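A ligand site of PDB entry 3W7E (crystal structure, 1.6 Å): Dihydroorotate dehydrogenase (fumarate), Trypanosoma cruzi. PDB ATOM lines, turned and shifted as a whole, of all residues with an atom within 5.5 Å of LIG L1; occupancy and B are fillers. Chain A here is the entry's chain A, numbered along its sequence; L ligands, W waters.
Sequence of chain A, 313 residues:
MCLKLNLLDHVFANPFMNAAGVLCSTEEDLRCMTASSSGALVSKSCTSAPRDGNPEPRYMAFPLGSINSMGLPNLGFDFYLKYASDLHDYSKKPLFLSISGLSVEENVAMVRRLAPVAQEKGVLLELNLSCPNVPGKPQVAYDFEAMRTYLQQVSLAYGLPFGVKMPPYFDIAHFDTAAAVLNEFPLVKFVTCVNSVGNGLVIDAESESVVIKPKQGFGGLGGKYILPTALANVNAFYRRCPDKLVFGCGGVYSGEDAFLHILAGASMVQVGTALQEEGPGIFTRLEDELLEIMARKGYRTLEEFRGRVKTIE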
ATOM      1  N   ALA A  19     -18.460   3.614   6.524  1.00  0.00           N
ATOM      2  CA  ALA A  19     -18.922   2.246   6.530  1.00  0.00           C
ATOM      3  C   ALA A  19     -19.919   2.048   7.681  1.00  0.00           C
ATOM      4  O   ALA A  19     -19.838   2.652   8.720  1.00  0.00           O
ATOM      5  CB  ALA A  19     -17.710   1.372   6.809  1.00  0.00           C
ATOM      6  N   ALA A  20     -20.936   1.220   7.462  1.00  0.00           N
ATOM      7  CA  ALA A  20     -21.926   0.999   8.432  1.00  0.00           C
ATOM      8  C   ALA A  20     -21.290   0.561   9.747  1.00  0.00           C
ATOM      9  O   ALA A  20     -20.341  -0.237   9.808  1.00  0.00           O
ATOM     10  CB  ALA A  20     -22.938  -0.059   8.028  1.00  0.00           C
ATOM     11  N   GLY A  21     -21.788   1.113  10.862  1.00  0.00           N
ATOM     12  CA  GLY A  21     -21.259   0.868  12.144  1.00  0.00           C
ATOM     13  C   GLY A  21     -20.315   1.925  12.725  1.00  0.00           C
ATOM     14  O   GLY A  21     -20.204   2.113  13.925  1.00  0.00           O
ATOM     15  N   VAL A  22     -19.703   2.672  11.835  1.00  0.00           N
ATOM     16  CA  VAL A  22     -18.716   3.712  12.242  1.00  0.00           C
ATOM     17  C   VAL A  22     -19.350   5.064  12.115  1.00  0.00           C
ATOM     18  O   VAL A  22     -19.864   5.483  11.060  1.00  0.00           O
ATOM     19  CB  VAL A  22     -17.473   3.610  11.376  1.00  0.00           C
ATOM     20  CG1 VAL A  22     -16.494   4.754  11.730  1.00  0.00           C
ATOM     21  CG2 VAL A  22     -16.856   2.231  11.635  1.00  0.00           C
ATOM     22  N   LYS A  44     -26.123   3.013  11.362  1.00  0.00           N
ATOM     23  CA  LYS A  44     -25.763   1.779  12.014  1.00  0.00           C
ATOM     24  C   LYS A  44     -26.778   0.689  11.704  1.00  0.00           C
ATOM     25  O   LYS A  44     -27.957   0.932  11.844  1.00  0.00           O
ATOM     26  CB  LYS A  44     -25.775   2.038  13.493  1.00  0.00           C
ATOM     27  CG  LYS A  44     -25.538   0.821  14.344  1.00  0.00           C
ATOM     28  CD  LYS A  44     -24.197   0.053  14.287  1.00  0.00           C
ATOM     29  CE  LYS A  44     -24.166  -1.376  14.835  1.00  0.00           C
ATOM     30  NZ  LYS A  44     -22.753  -2.086  14.776  1.00  0.00           N
ATOM     31  N   SER A  45     -26.312  -0.505  11.338  1.00  0.00           N
ATOM     32  CA  SER A  45     -27.211  -1.675  11.076  1.00  0.00           C
ATOM     33  C   SER A  45     -28.083  -1.819  12.332  1.00  0.00           C
ATOM     34  O   SER A  45     -27.567  -1.832  13.441  1.00  0.00           O
ATOM     35  CB  SER A  45     -26.458  -2.977  10.904  1.00  0.00           C
ATOM     36  OG  SER A  45     -25.717  -2.929   9.702  1.00  0.00           O
ATOM     37  N   TYR A  59     -14.022  -3.147  20.767  1.00  0.00           N
ATOM     38  CA  TYR A  59     -13.287  -2.649  19.588  1.00  0.00           C
ATOM     39  C   TYR A  59     -11.934  -2.250  20.032  1.00  0.00           C
ATOM     40  O   TYR A  59     -11.771  -1.580  21.049  1.00  0.00           O
ATOM     41  CB  TYR A  59     -14.046  -1.431  19.022  1.00  0.00           C
ATOM     42  CG  TYR A  59     -13.288  -0.653  17.929  1.00  0.00           C
ATOM     43  CD1 TYR A  59     -13.325  -1.021  16.591  1.00  0.00           C
ATOM     44  CD2 TYR A  59     -12.425   0.410  18.266  1.00  0.00           C
ATOM     45  CE1 TYR A  59     -12.569  -0.343  15.641  1.00  0.00           C
ATOM     46  CE2 TYR A  59     -11.700   1.055  17.345  1.00  0.00           C
ATOM     47  CZ  TYR A  59     -11.734   0.707  16.027  1.00  0.00           C
ATOM     48  OH  TYR A  59     -11.046   1.375  15.040  1.00  0.00           O
ATOM     49  N   SER A  66      -8.110  -2.973  12.714  1.00  0.00           N
ATOM     50  CA  SER A  66      -8.964  -3.038  13.916  1.00  0.00           C
ATOM     51  C   SER A  66      -9.573  -4.490  14.045  1.00  0.00           C
ATOM     52  O   SER A  66      -9.612  -5.259  13.064  1.00  0.00           O
ATOM     53  CB  SER A  66     -10.096  -2.002  13.822  1.00  0.00           C
ATOM     54  OG  SER A  66     -11.030  -2.358  12.823  1.00  0.00           O
ATOM     55  N   ASN A  68     -13.182  -6.121  16.061  1.00  0.00           N
ATOM     56  CA  ASN A  68     -14.339  -5.784  16.824  1.00  0.00           C
ATOM     57  C   ASN A  68     -15.252  -6.976  16.974  1.00  0.00           C
ATOM     58  O   ASN A  68     -15.452  -7.779  16.078  1.00  0.00           O
ATOM     59  CB  ASN A  68     -15.103  -4.599  16.242  1.00  0.00           C
ATOM     60  CG  ASN A  68     -16.103  -4.969  15.147  1.00  0.00           C
ATOM     61  OD1 ASN A  68     -17.276  -5.322  15.424  1.00  0.00           O
ATOM     62  ND2 ASN A  68     -15.701  -4.850  13.890  1.00  0.00           N
ATOM     63  N   MET A  70     -18.692  -6.010  18.314  1.00  0.00           N
ATOM     64  CA  MET A  70     -19.546  -5.055  18.970  1.00  0.00           C
ATOM     65  C   MET A  70     -20.821  -5.658  19.479  1.00  0.00           C
ATOM     66  O   MET A  70     -21.315  -5.156  20.492  1.00  0.00           O
ATOM     67  CB  MET A  70     -19.876  -3.947  17.993  1.00  0.00           C
ATOM     68  CG  MET A  70     -18.786  -3.091  17.397  1.00  0.00           C
ATOM     69  SD  MET A  70     -17.748  -2.287  18.581  1.00  0.00           S
ATOM     70  CE  MET A  70     -18.810  -1.035  19.170  1.00  0.00           C
ATOM     71  N   LEU A  72     -23.745  -5.691  17.664  1.00  0.00           N
ATOM     72  CA  LEU A  72     -24.806  -4.882  17.084  1.00  0.00           C
ATOM     73  C   LEU A  72     -25.519  -3.955  18.137  1.00  0.00           C
ATOM     74  O   LEU A  72     -26.738  -3.833  18.173  1.00  0.00           O
ATOM     75  CB  LEU A  72     -25.827  -5.715  16.271  1.00  0.00           C
ATOM     76  CG  LEU A  72     -26.552  -4.807  15.250  1.00  0.00           C
ATOM     77  CD1 LEU A  72     -25.777  -4.715  13.956  1.00  0.00           C
ATOM     78  CD2 LEU A  72     -27.992  -5.266  15.006  1.00  0.00           C
ATOM     79  N   SER A  98     -29.039   1.126   7.053  1.00  0.00           N
ATOM     80  CA  SER A  98     -28.669  -0.314   7.138  1.00  0.00           C
ATOM     81  C   SER A  98     -29.507  -1.085   8.097  1.00  0.00           C
ATOM     82  O   SER A  98     -29.789  -0.625   9.201  1.00  0.00           O
ATOM     83  CB  SER A  98     -27.222  -0.522   7.509  1.00  0.00           C
ATOM     84  OG  SER A  98     -26.893  -1.908   7.588  1.00  0.00           O
ATOM     85  N   GLU A 126     -29.560  -0.546   2.741  1.00  0.00           N
ATOM     86  CA  GLU A 126     -28.441  -1.510   2.693  1.00  0.00           C
ATOM     87  C   GLU A 126     -28.762  -2.637   3.656  1.00  0.00           C
ATOM     88  O   GLU A 126     -28.825  -2.458   4.889  1.00  0.00           O
ATOM     89  CB  GLU A 126     -27.071  -0.857   2.999  1.00  0.00           C
ATOM     90  CG  GLU A 126     -25.889  -1.818   2.854  1.00  0.00           C
ATOM     91  CD  GLU A 126     -24.544  -1.064   3.063  1.00  0.00           C
ATOM     92  OE1 GLU A 126     -24.135  -1.002   4.240  1.00  0.00           O
ATOM     93  OE2 GLU A 126     -23.881  -0.580   2.124  1.00  0.00           O
ATOM     94  N   ASN A 128     -27.720  -5.850   5.599  1.00  0.00           N
ATOM     95  CA  ASN A 128     -26.516  -6.514   6.043  1.00  0.00           C
ATOM     96  C   ASN A 128     -26.767  -7.981   6.146  1.00  0.00           C
ATOM     97  O   ASN A 128     -27.406  -8.424   7.109  1.00  0.00           O
ATOM     98  CB  ASN A 128     -26.070  -5.843   7.348  1.00  0.00           C
ATOM     99  CG  ASN A 128     -24.870  -6.461   7.980  1.00  0.00           C
ATOM    100  OD1 ASN A 128     -24.288  -7.276   7.430  1.00  0.00           O
ATOM    101  ND2 ASN A 128     -24.541  -5.959   9.165  1.00  0.00           N
ATOM    102  N   LYS A 165     -24.956  -5.695   1.872  1.00  0.00           N
ATOM    103  CA  LYS A 165     -23.578  -5.677   2.414  1.00  0.00           C
ATOM    104  C   LYS A 165     -23.121  -7.087   2.613  1.00  0.00           C
ATOM    105  O   LYS A 165     -23.800  -7.915   3.273  1.00  0.00           O
ATOM    106  CB  LYS A 165     -23.569  -4.930   3.749  1.00  0.00           C
ATOM    107  CG  LYS A 165     -22.223  -4.854   4.483  1.00  0.00           C
ATOM    108  CD  LYS A 165     -21.271  -3.914   3.849  1.00  0.00           C
ATOM    109  CE  LYS A 165     -20.098  -3.704   4.785  1.00  0.00           C
ATOM    110  NZ  LYS A 165     -20.432  -2.880   5.927  1.00  0.00           N
ATOM    111  N   VAL A 194     -16.472  -4.998   1.268  1.00  0.00           N
ATOM    112  CA  VAL A 194     -16.804  -6.106   2.133  1.00  0.00           C
ATOM    113  C   VAL A 194     -17.055  -5.640   3.581  1.00  0.00           C
ATOM    114  O   VAL A 194     -16.520  -4.612   4.039  1.00  0.00           O
ATOM    115  CB  VAL A 194     -15.707  -7.211   2.181  1.00  0.00           C
ATOM    116  CG1 VAL A 194     -15.561  -7.820   0.817  1.00  0.00           C
ATOM    117  CG2 VAL A 194     -14.356  -6.598   2.623  1.00  0.00           C
ATOM    118  N   ASN A 195     -17.800  -6.457   4.283  1.00  0.00           N
ATOM    119  CA  ASN A 195     -17.797  -6.491   5.751  1.00  0.00           C
ATOM    120  C   ASN A 195     -16.435  -6.982   6.314  1.00  0.00           C
ATOM    121  O   ASN A 195     -15.531  -7.323   5.523  1.00  0.00           O
ATOM    122  CB  ASN A 195     -18.979  -7.338   6.265  1.00  0.00           C
ATOM    123  CG  ASN A 195     -19.612  -6.787   7.531  1.00  0.00           C
ATOM    124  OD1 ASN A 195     -18.908  -6.405   8.457  1.00  0.00           O
ATOM    125  ND2 ASN A 195     -20.952  -6.683   7.538  1.00  0.00           N
ATOM    126  N   SER A 196     -16.300  -6.998   7.635  1.00  0.00           N
ATOM    127  CA  SER A 196     -15.058  -7.379   8.283  1.00  0.00           C
ATOM    128  C   SER A 196     -14.675  -8.842   8.033  1.00  0.00           C
ATOM    129  O   SER A 196     -15.533  -9.723   7.999  1.00  0.00           O
ATOM    130  CB  SER A 196     -15.126  -7.115   9.788  1.00  0.00           C
ATOM    131  OG  SER A 196     -16.365  -7.549  10.332  1.00  0.00           O
ATOM    132  N   LEU A 221     -12.076  -8.297  11.479  1.00  0.00           N
ATOM    133  CA  LEU A 221     -10.930  -7.454  11.199  1.00  0.00           C
ATOM    134  C   LEU A 221     -11.281  -6.455  10.113  1.00  0.00           C
ATOM    135  O   LEU A 221     -11.923  -6.787   9.073  1.00  0.00           O
ATOM    136  CB  LEU A 221      -9.787  -8.315  10.585  1.00  0.00           C
ATOM    137  CG  LEU A 221      -9.280  -9.467  11.500  1.00  0.00           C
ATOM    138  CD1 LEU A 221      -8.271 -10.336  10.736  1.00  0.00           C
ATOM    139  CD2 LEU A 221      -8.731  -8.949  12.798  1.00  0.00           C
ATOM    140  N   GLY A 222     -10.757  -5.259  10.301  1.00  0.00           N
ATOM    141  CA  GLY A 222     -10.824  -4.189   9.311  1.00  0.00           C
ATOM    142  C   GLY A 222      -9.480  -3.522   9.160  1.00  0.00           C
ATOM    143  O   GLY A 222      -8.538  -3.772   9.949  1.00  0.00           O
ATOM    144  N   GLY A 223      -9.387  -2.645   8.222  1.00  0.00           N
ATOM    145  CA  GLY A 223      -8.243  -1.838   8.050  1.00  0.00           C
ATOM    146  C   GLY A 223      -7.197  -2.368   7.058  1.00  0.00           C
ATOM    147  O   GLY A 223      -7.502  -3.103   6.126  1.00  0.00           O
ATOM    148  N   ILE A 226      -6.944  -5.895   5.419  1.00  0.00           N
ATOM    149  CA  ILE A 226      -7.932  -6.502   4.584  1.00  0.00           C
ATOM    150  C   ILE A 226      -8.063  -5.836   3.162  1.00  0.00           C
ATOM    151  O   ILE A 226      -8.932  -6.256   2.429  1.00  0.00           O
ATOM    152  CB  ILE A 226      -9.329  -6.545   5.251  1.00  0.00           C
ATOM    153  CG1 ILE A 226     -10.091  -5.207   5.235  1.00  0.00           C
ATOM    154  CG2 ILE A 226      -9.312  -7.085   6.660  1.00  0.00           C
ATOM    155  CD1 ILE A 226     -11.608  -5.249   5.468  1.00  0.00           C
ATOM    156  N   CYS A 249     -15.641  -1.368   0.228  1.00  0.00           N
ATOM    157  CA  CYS A 249     -15.373  -1.129   1.661  1.00  0.00           C
ATOM    158  C   CYS A 249     -14.248  -2.032   2.068  1.00  0.00           C
ATOM    159  O   CYS A 249     -14.271  -3.204   1.757  1.00  0.00           O
ATOM    160  CB  CYS A 249     -16.594  -1.386   2.470  1.00  0.00           C
ATOM    161  SG  CYS A 249     -16.506  -0.885   4.191  1.00  0.00           S
ATOM    162  N   GLY A 250     -13.248  -1.494   2.717  1.00  0.00           N
ATOM    163  CA  GLY A 250     -12.183  -2.225   3.369  1.00  0.00           C
ATOM    164  C   GLY A 250     -10.805  -1.673   3.084  1.00  0.00           C
ATOM    165  O   GLY A 250     -10.374  -1.621   1.940  1.00  0.00           O
ATOM    166  N   GLY A 251     -10.127  -1.359   4.177  1.00  0.00           N
ATOM    167  CA  GLY A 251      -8.755  -0.887   4.026  1.00  0.00           C
ATOM    168  C   GLY A 251      -8.504   0.471   3.463  1.00  0.00           C
ATOM    169  O   GLY A 251      -7.398   0.716   3.014  1.00  0.00           O
ATOM    170  N   VAL A 252      -9.527   1.325   3.339  1.00  0.00           N
ATOM    171  CA  VAL A 252      -9.272   2.663   2.785  1.00  0.00           C
ATOM    172  C   VAL A 252      -8.739   3.615   3.838  1.00  0.00           C
ATOM    173  O   VAL A 252      -9.507   3.915   4.796  1.00  0.00           O
ATOM    174  CB  VAL A 252     -10.532   3.254   2.090  1.00  0.00           C
ATOM    175  CG1 VAL A 252     -10.365   4.688   1.609  1.00  0.00           C
ATOM    176  CG2 VAL A 252     -11.019   2.343   0.966  1.00  0.00           C
ATOM    177  N   GLN A 270     -16.507   3.228   0.905  1.00  0.00           N
ATOM    178  CA  GLN A 270     -16.882   3.393   2.286  1.00  0.00           C
ATOM    179  C   GLN A 270     -15.565   3.301   3.145  1.00  0.00           C
ATOM    180  O   GLN A 270     -14.623   2.568   2.756  1.00  0.00           O
ATOM    181  CB  GLN A 270     -17.840   2.300   2.691  1.00  0.00           C
ATOM    182  CG  GLN A 270     -19.049   2.172   1.850  1.00  0.00           C
ATOM    183  CD  GLN A 270     -20.109   1.256   2.400  1.00  0.00           C
ATOM    184  OE1 GLN A 270     -19.821   0.342   3.189  1.00  0.00           O
ATOM    185  NE2 GLN A 270     -21.342   1.440   1.971  1.00  0.00           N
ATOM    186  N   VAL A 271     -15.595   3.964   4.329  1.00  0.00           N
ATOM    187  CA  VAL A 271     -14.442   4.075   5.167  1.00  0.00           C
ATOM    188  C   VAL A 271     -14.885   3.767   6.574  1.00  0.00           C
ATOM    189  O   VAL A 271     -15.734   4.436   7.163  1.00  0.00           O
ATOM    190  CB  VAL A 271     -13.889   5.532   5.064  1.00  0.00           C
ATOM    191  CG1 VAL A 271     -12.593   5.683   5.863  1.00  0.00           C
ATOM    192  CG2 VAL A 271     -13.723   5.979   3.601  1.00  0.00           C
ATOM    193  N   GLY A 272     -14.262   2.737   7.129  1.00  0.00           N
ATOM    194  CA  GLY A 272     -14.641   2.204   8.446  1.00  0.00           C
ATOM    195  C   GLY A 272     -13.510   2.558   9.429  1.00  0.00           C
ATOM    196  O   GLY A 272     -13.496   3.651  10.006  1.00  0.00           O
ATOM    197  N   THR A 273     -12.586   1.608   9.649  1.00  0.00           N
ATOM    198  CA  THR A 273     -11.526   1.719  10.637  1.00  0.00           C
ATOM    199  C   THR A 273     -10.808   3.065  10.513  1.00  0.00           C
ATOM    200  O   THR A 273     -10.582   3.737  11.505  1.00  0.00           O
ATOM    201  CB  THR A 273     -10.510   0.598  10.414  1.00  0.00           C
ATOM    202  OG1 THR A 273     -11.143  -0.684  10.639  1.00  0.00           O
ATOM    203  CG2 THR A 273      -9.337   0.711  11.347  1.00  0.00           C
ATOM    204  N   ALA A 274     -10.429   3.488   9.306  1.00  0.00           N
ATOM    205  CA  ALA A 274      -9.646   4.760   9.234  1.00  0.00           C
ATOM    206  C   ALA A 274     -10.470   5.960   9.726  1.00  0.00           C
ATOM    207  O   ALA A 274      -9.882   6.910  10.242  1.00  0.00           O
ATOM    208  CB  ALA A 274      -9.131   4.946   7.814  1.00  0.00           C
ATOM    209  N   GLN A 276     -12.993   5.726  12.011  1.00  0.00           N
ATOM    210  CA  GLN A 276     -13.058   5.541  13.442  1.00  0.00           C
ATOM    211  C   GLN A 276     -11.795   6.056  14.133  1.00  0.00           C
ATOM    212  O   GLN A 276     -11.871   6.709  15.184  1.00  0.00           O
ATOM    213  CB  GLN A 276     -13.190   4.068  13.751  1.00  0.00           C
ATOM    214  CG  GLN A 276     -13.277   3.723  15.237  1.00  0.00           C
ATOM    215  CD  GLN A 276     -14.412   4.419  15.998  1.00  0.00           C
ATOM    216  OE1 GLN A 276     -14.259   4.865  17.183  1.00  0.00           O
ATOM    217  NE2 GLN A 276     -15.506   4.505  15.406  1.00  0.00           N
HETATM  218  N1  LIG L   1     -20.800  -3.426   9.025  1.00  0.00           N
HETATM  219  C1  LIG L   1     -22.129  -3.424   8.881  1.00  0.00           C
HETATM  220  O1  LIG L   1     -22.582  -3.635   7.740  1.00  0.00           O
HETATM  221  N2  LIG L   1     -22.986  -3.018   9.870  1.00  0.00           N
HETATM  222  C2  LIG L   1     -22.578  -2.659  11.102  1.00  0.00           C
HETATM  223  O2  LIG L   1     -23.331  -2.307  12.014  1.00  0.00           O
HETATM  224  C3  LIG L   1     -21.140  -2.691  11.358  1.00  0.00           C
HETATM  225  N3  LIG L   1     -20.631  -2.270  12.507  1.00  0.00           N
HETATM  226  C4  LIG L   1     -19.318  -2.119  12.662  1.00  0.00           C
HETATM  227  C5  LIG L   1     -18.778  -1.506  13.824  1.00  0.00           C
HETATM  228  C6  LIG L   1     -17.419  -1.311  13.967  1.00  0.00           C
HETATM  229  C7  LIG L   1     -16.926  -0.707  15.311  1.00  0.00           C
HETATM  230  C8  LIG L   1     -16.545  -1.610  12.867  1.00  0.00           C
HETATM  231  C9  LIG L   1     -15.098  -1.396  12.981  1.00  0.00           C
HETATM  232  C10 LIG L   1     -17.039  -2.184  11.706  1.00  0.00           C
HETATM  233  C11 LIG L   1     -18.384  -2.404  11.556  1.00  0.00           C
HETATM  234  N4  LIG L   1     -18.943  -2.942  10.393  1.00  0.00           N
HETATM  235  C12 LIG L   1     -20.293  -3.039  10.209  1.00  0.00           C
HETATM  236  C13 LIG L   1     -18.089  -3.243   9.256  1.00  0.00           C
HETATM  237  C14 LIG L   1     -17.639  -2.067   8.462  1.00  0.00           C
HETATM  238  O3  LIG L   1     -18.821  -1.476   7.874  1.00  0.00           O
HETATM  239  C15 LIG L   1     -16.658  -2.396   7.350  1.00  0.00           C
HETATM  240  O4  LIG L   1     -17.327  -3.331   6.490  1.00  0.00           O
HETATM  241  C16 LIG L   1     -15.393  -3.097   7.892  1.00  0.00           C
HETATM  242  O5  LIG L   1     -14.913  -2.418   9.080  1.00  0.00           O
HETATM  243  C17 LIG L   1     -14.317  -3.002   6.798  1.00  0.00           C
HETATM  244  O6  LIG L   1     -13.925  -1.698   6.435  1.00  0.00           O
HETATM  245  P1  LIG L   1     -12.612  -0.953   7.015  1.00  0.00           P
HETATM  246  O7  LIG L   1     -12.668   0.437   6.429  1.00  0.00           O
HETATM  247  O8  LIG L   1     -11.433  -1.780   6.592  1.00  0.00           O
HETATM  248  O9  LIG L   1     -12.776  -0.950   8.529  1.00  0.00           O
HETATM  249  O1  LG2 L   2     -20.368  -6.723  15.812  1.00  0.00           O
HETATM  250  C1  LG2 L   2     -21.082  -6.011  15.119  1.00  0.00           C
HETATM  251  O2  LG2 L   2     -21.874  -5.161  15.533  1.00  0.00           O
HETATM  252  C2  LG2 L   2     -20.706  -6.034  13.665  1.00  0.00           C
HETATM  253  N1  LG2 L   2     -19.344  -5.711  13.402  1.00  0.00           N
HETATM  254  C3  LG2 L   2     -18.849  -5.755  12.098  1.00  0.00           C
HETATM  255  O3  LG2 L   2     -17.662  -5.592  11.859  1.00  0.00           O
HETATM  256  N2  LG2 L   2     -19.766  -6.027  11.092  1.00  0.00           N
HETATM  257  C4  LG2 L   2     -21.147  -6.244  11.332  1.00  0.00           C
HETATM  258  O4  LG2 L   2     -21.874  -6.449  10.342  1.00  0.00           O
HETATM  259  C5  LG2 L   2     -21.576  -6.316  12.690  1.00  0.00           C
HETATM  260  C6  LG2 L   2     -22.932  -6.675  12.958  1.00  0.00           C
HETATM  261  C7  LG2 L   2     -23.221  -8.206  12.636  1.00  0.00           C
HETATM  262  C8  LG2 L   2     -24.548  -8.511  13.290  1.00  0.00           C
HETATM  263  C9  LG2 L   2     -24.589  -8.988  14.667  1.00  0.00           C
HETATM  264  C10 LG2 L   2     -23.419  -9.264  15.345  1.00  0.00           C
HETATM  265  C11 LG2 L   2     -23.484  -9.705  16.659  1.00  0.00           C
HETATM  266  O5  LG2 L   2     -22.299  -9.934  17.378  1.00  0.00           O
HETATM  267  C12 LG2 L   2     -20.911  -9.719  16.925  1.00  0.00           C
HETATM  268  C13 LG2 L   2     -24.775  -9.884  17.169  1.00  0.00           C
HETATM  269  C14 LG2 L   2     -25.922  -9.644  16.553  1.00  0.00           C
HETATM  270  C15 LG2 L   2     -25.877  -9.171  15.241  1.00  0.00           C
HETATM  271  C16 LG2 L   2     -27.066  -8.936  14.517  1.00  0.00           C
HETATM  272  C17 LG2 L   2     -27.087  -8.507  13.181  1.00  0.00           C
HETATM  273  C18 LG2 L   2     -25.774  -8.283  12.631  1.00  0.00           C
HETATM  274  O   HOH W   1     -12.514   1.035   3.829  1.00  0.00           O
HETATM  275  O   HOH W   2     -20.958   0.064  15.981  1.00  0.00           O
HETATM  276  O   HOH W   3     -14.309  -4.484  10.587  1.00  0.00           O
HETATM  277  O   HOH W   4     -24.808  -2.709   6.177  1.00  0.00           O
HETATM  278  O   HOH W   5     -10.564   2.123   6.813  1.00  0.00           O
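O9 of LIG L1 is in hydrogen-bond range of N of Thr 273 (2.8 Å). The side-chain amino group of Lys 44 lies within hydrogen-bond range of an oxygen (O2) of LIG L1, at 2.8 Å. An oxygen (O1) of LIG L1 lies within hydrogen-bond range of the side-chain amide nitrogen of Asn 128, at 3.4 Å. The backbone NH (N) of Gly 251 is in hydrogen-bond range of an oxygen (O8) of LIG L1 (2.8 Å). An oxygen (O2) of LG2 L2 lies within salt-bridge range of the side-chain amino group (NZ) of Lys 44, 3.3 Å away. O8 of LIG L1 lies within hydrogen-bond range of N of Gly 223, at 2.8 Å. The side-chain amide nitrogen (ND2) of Asn 128 lies within hydrogen-bond range of an oxygen (O4) of LG2 L2, 3.0 Å away. An oxygen (O2) of LG2 L2 sits at hydrogen-bond distance from the backbone NH (N) of Leu 72 (2.9 Å). An oxygen (O3) of LIG L1 is in hydrogen-bond range of the backbone NH (N) of Ala 20 (3.5 Å). The side-chain hydroxyl (OG1) of Thr 273 is in hydrogen-bond range of an oxygen (O9) of LIG L1 (2.7 Å). An oxygen (O4) of LIG L1 sits at hydrogen-bond distance from the side-chain sulfur (SG) of Cys 249, at 3.5 Å. An oxygen (O3) of LG2 L2 sits at hydrogen-bond distance from the side-chain hydroxyl (OG) of Ser 196, at 2.8 Å. The side-chain amide oxygen (OD1) of Asn 68 lies within hydrogen-bond range of a nitrogen (N1) of LG2 L2 (2.9 Å). N of Gly 272 is in hydrogen-bond range of O7 of LIG L1, at 2.9 Å. N of Met 70 is in hydrogen-bond range of O1 of LG2 L2 (3.1 Å). OD1 of Asn 195 lies within hydrogen-bond range of N2 of LG2 L2, 2.8 Å away. The side-chain hydroxyl (OG) of Ser 45 sits at hydrogen-bond distance from a nitrogen (N2) of LIG L1 (2.7 Å). O of Val 194 is in hydrogen-bond range of O4 of LIG L1 (2.9 Å). The side-chain amino group (NZ) of Lys 165 is in hydrogen-bond range of an oxygen (O3) of LIG L1. O of Ala 20 lies within hydrogen-bond range of O3 of LIG L1, at 2.8 Å. The side-chain amide nitrogen (ND2) of Asn 195 lies within hydrogen-bond range of an oxygen (O1) of LIG L1 (3.5 Å).
A nitrogen (N1) of LIG L1 lies close to a nitrogen (N2) of LG2 L2 (3.5 Å).
ND2 of Asn 195 lies within hydrogen-bond range of OD1 of Asn 128 (3.4 Å). The side-chain hydroxyl of Ser 45 is in hydrogen-bond range of the side-chain amide nitrogen of Asn 128 (3.3 Å). SG of Cys 249 is in hydrogen-bond range of OE1 of Gln 270 (3.7 Å). The backbone NH of Ser 66 is in hydrogen-bond range of the backbone carbonyl oxygen of Gly 222 (2.9 Å). OD1 of Asn 195 lies within hydrogen-bond range of OG of Ser 196. The backbone NH (N) of Met 70 lies within hydrogen-bond range of the side-chain amide oxygen (OD1) of Asn 68 (3.3 Å). The backbone NH (N) of Ala 19 lies within hydrogen-bond range of the backbone carbonyl oxygen (O) of Val 271 (2.9 Å). The backbone carbonyl oxygen of Cys 249 sits at hydrogen-bond distance from the backbone NH of Val 194 (2.9 Å).
Merely in contact with LIG L1: Gly 21 (3.2 Å), Ala 19 (3.2 Å), Gly 250 (3.3 Å), Asn 68 (3.5 Å), Ile 226 (3.7 Å), Gly 222 (3.7 Å), Met 70 (3.7 Å), Tyr 59 (3.8 Å), Leu 72 (3.9 Å) and Ser 196 (3.98 Å). Within 4 Å of LIG L1: Ala 19, Ala 20, Gly 21, Lys 44, Ser 45, Tyr 59, Asn 68, Met 70, Leu 72, Asn 128, Lys 165, Val 194, Asn 195, Ser 196, Gly 222, Gly 223, Ile 226, Cys 249, Gly 250, Gly 251, Gly 272 and Thr 273. The nearest printed residue that does not touch LIG L1 is Val 271 (4.003 Å).
Water W5 lies within hydrogen-bond range of an oxygen (O7) of LIG L1 (2.7 Å), the backbone NH of Ala 274 (2.8 Å) and the backbone carbonyl oxygen of Val 252 (2.9 Å). Water W4 lies within hydrogen-bond range of the side-chain hydroxyl of Ser 98 (2.6 Å), the side-chain carboxylate of Glu 126 (2.7 Å) and an oxygen (O1) of LIG L1 (2.9 Å). Water W2 bridges the backbone carbonyl oxygen (O) of Gly 21 (3.0 Å) and the side-chain amino group (NZ) of Lys 44 (3.0 Å).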
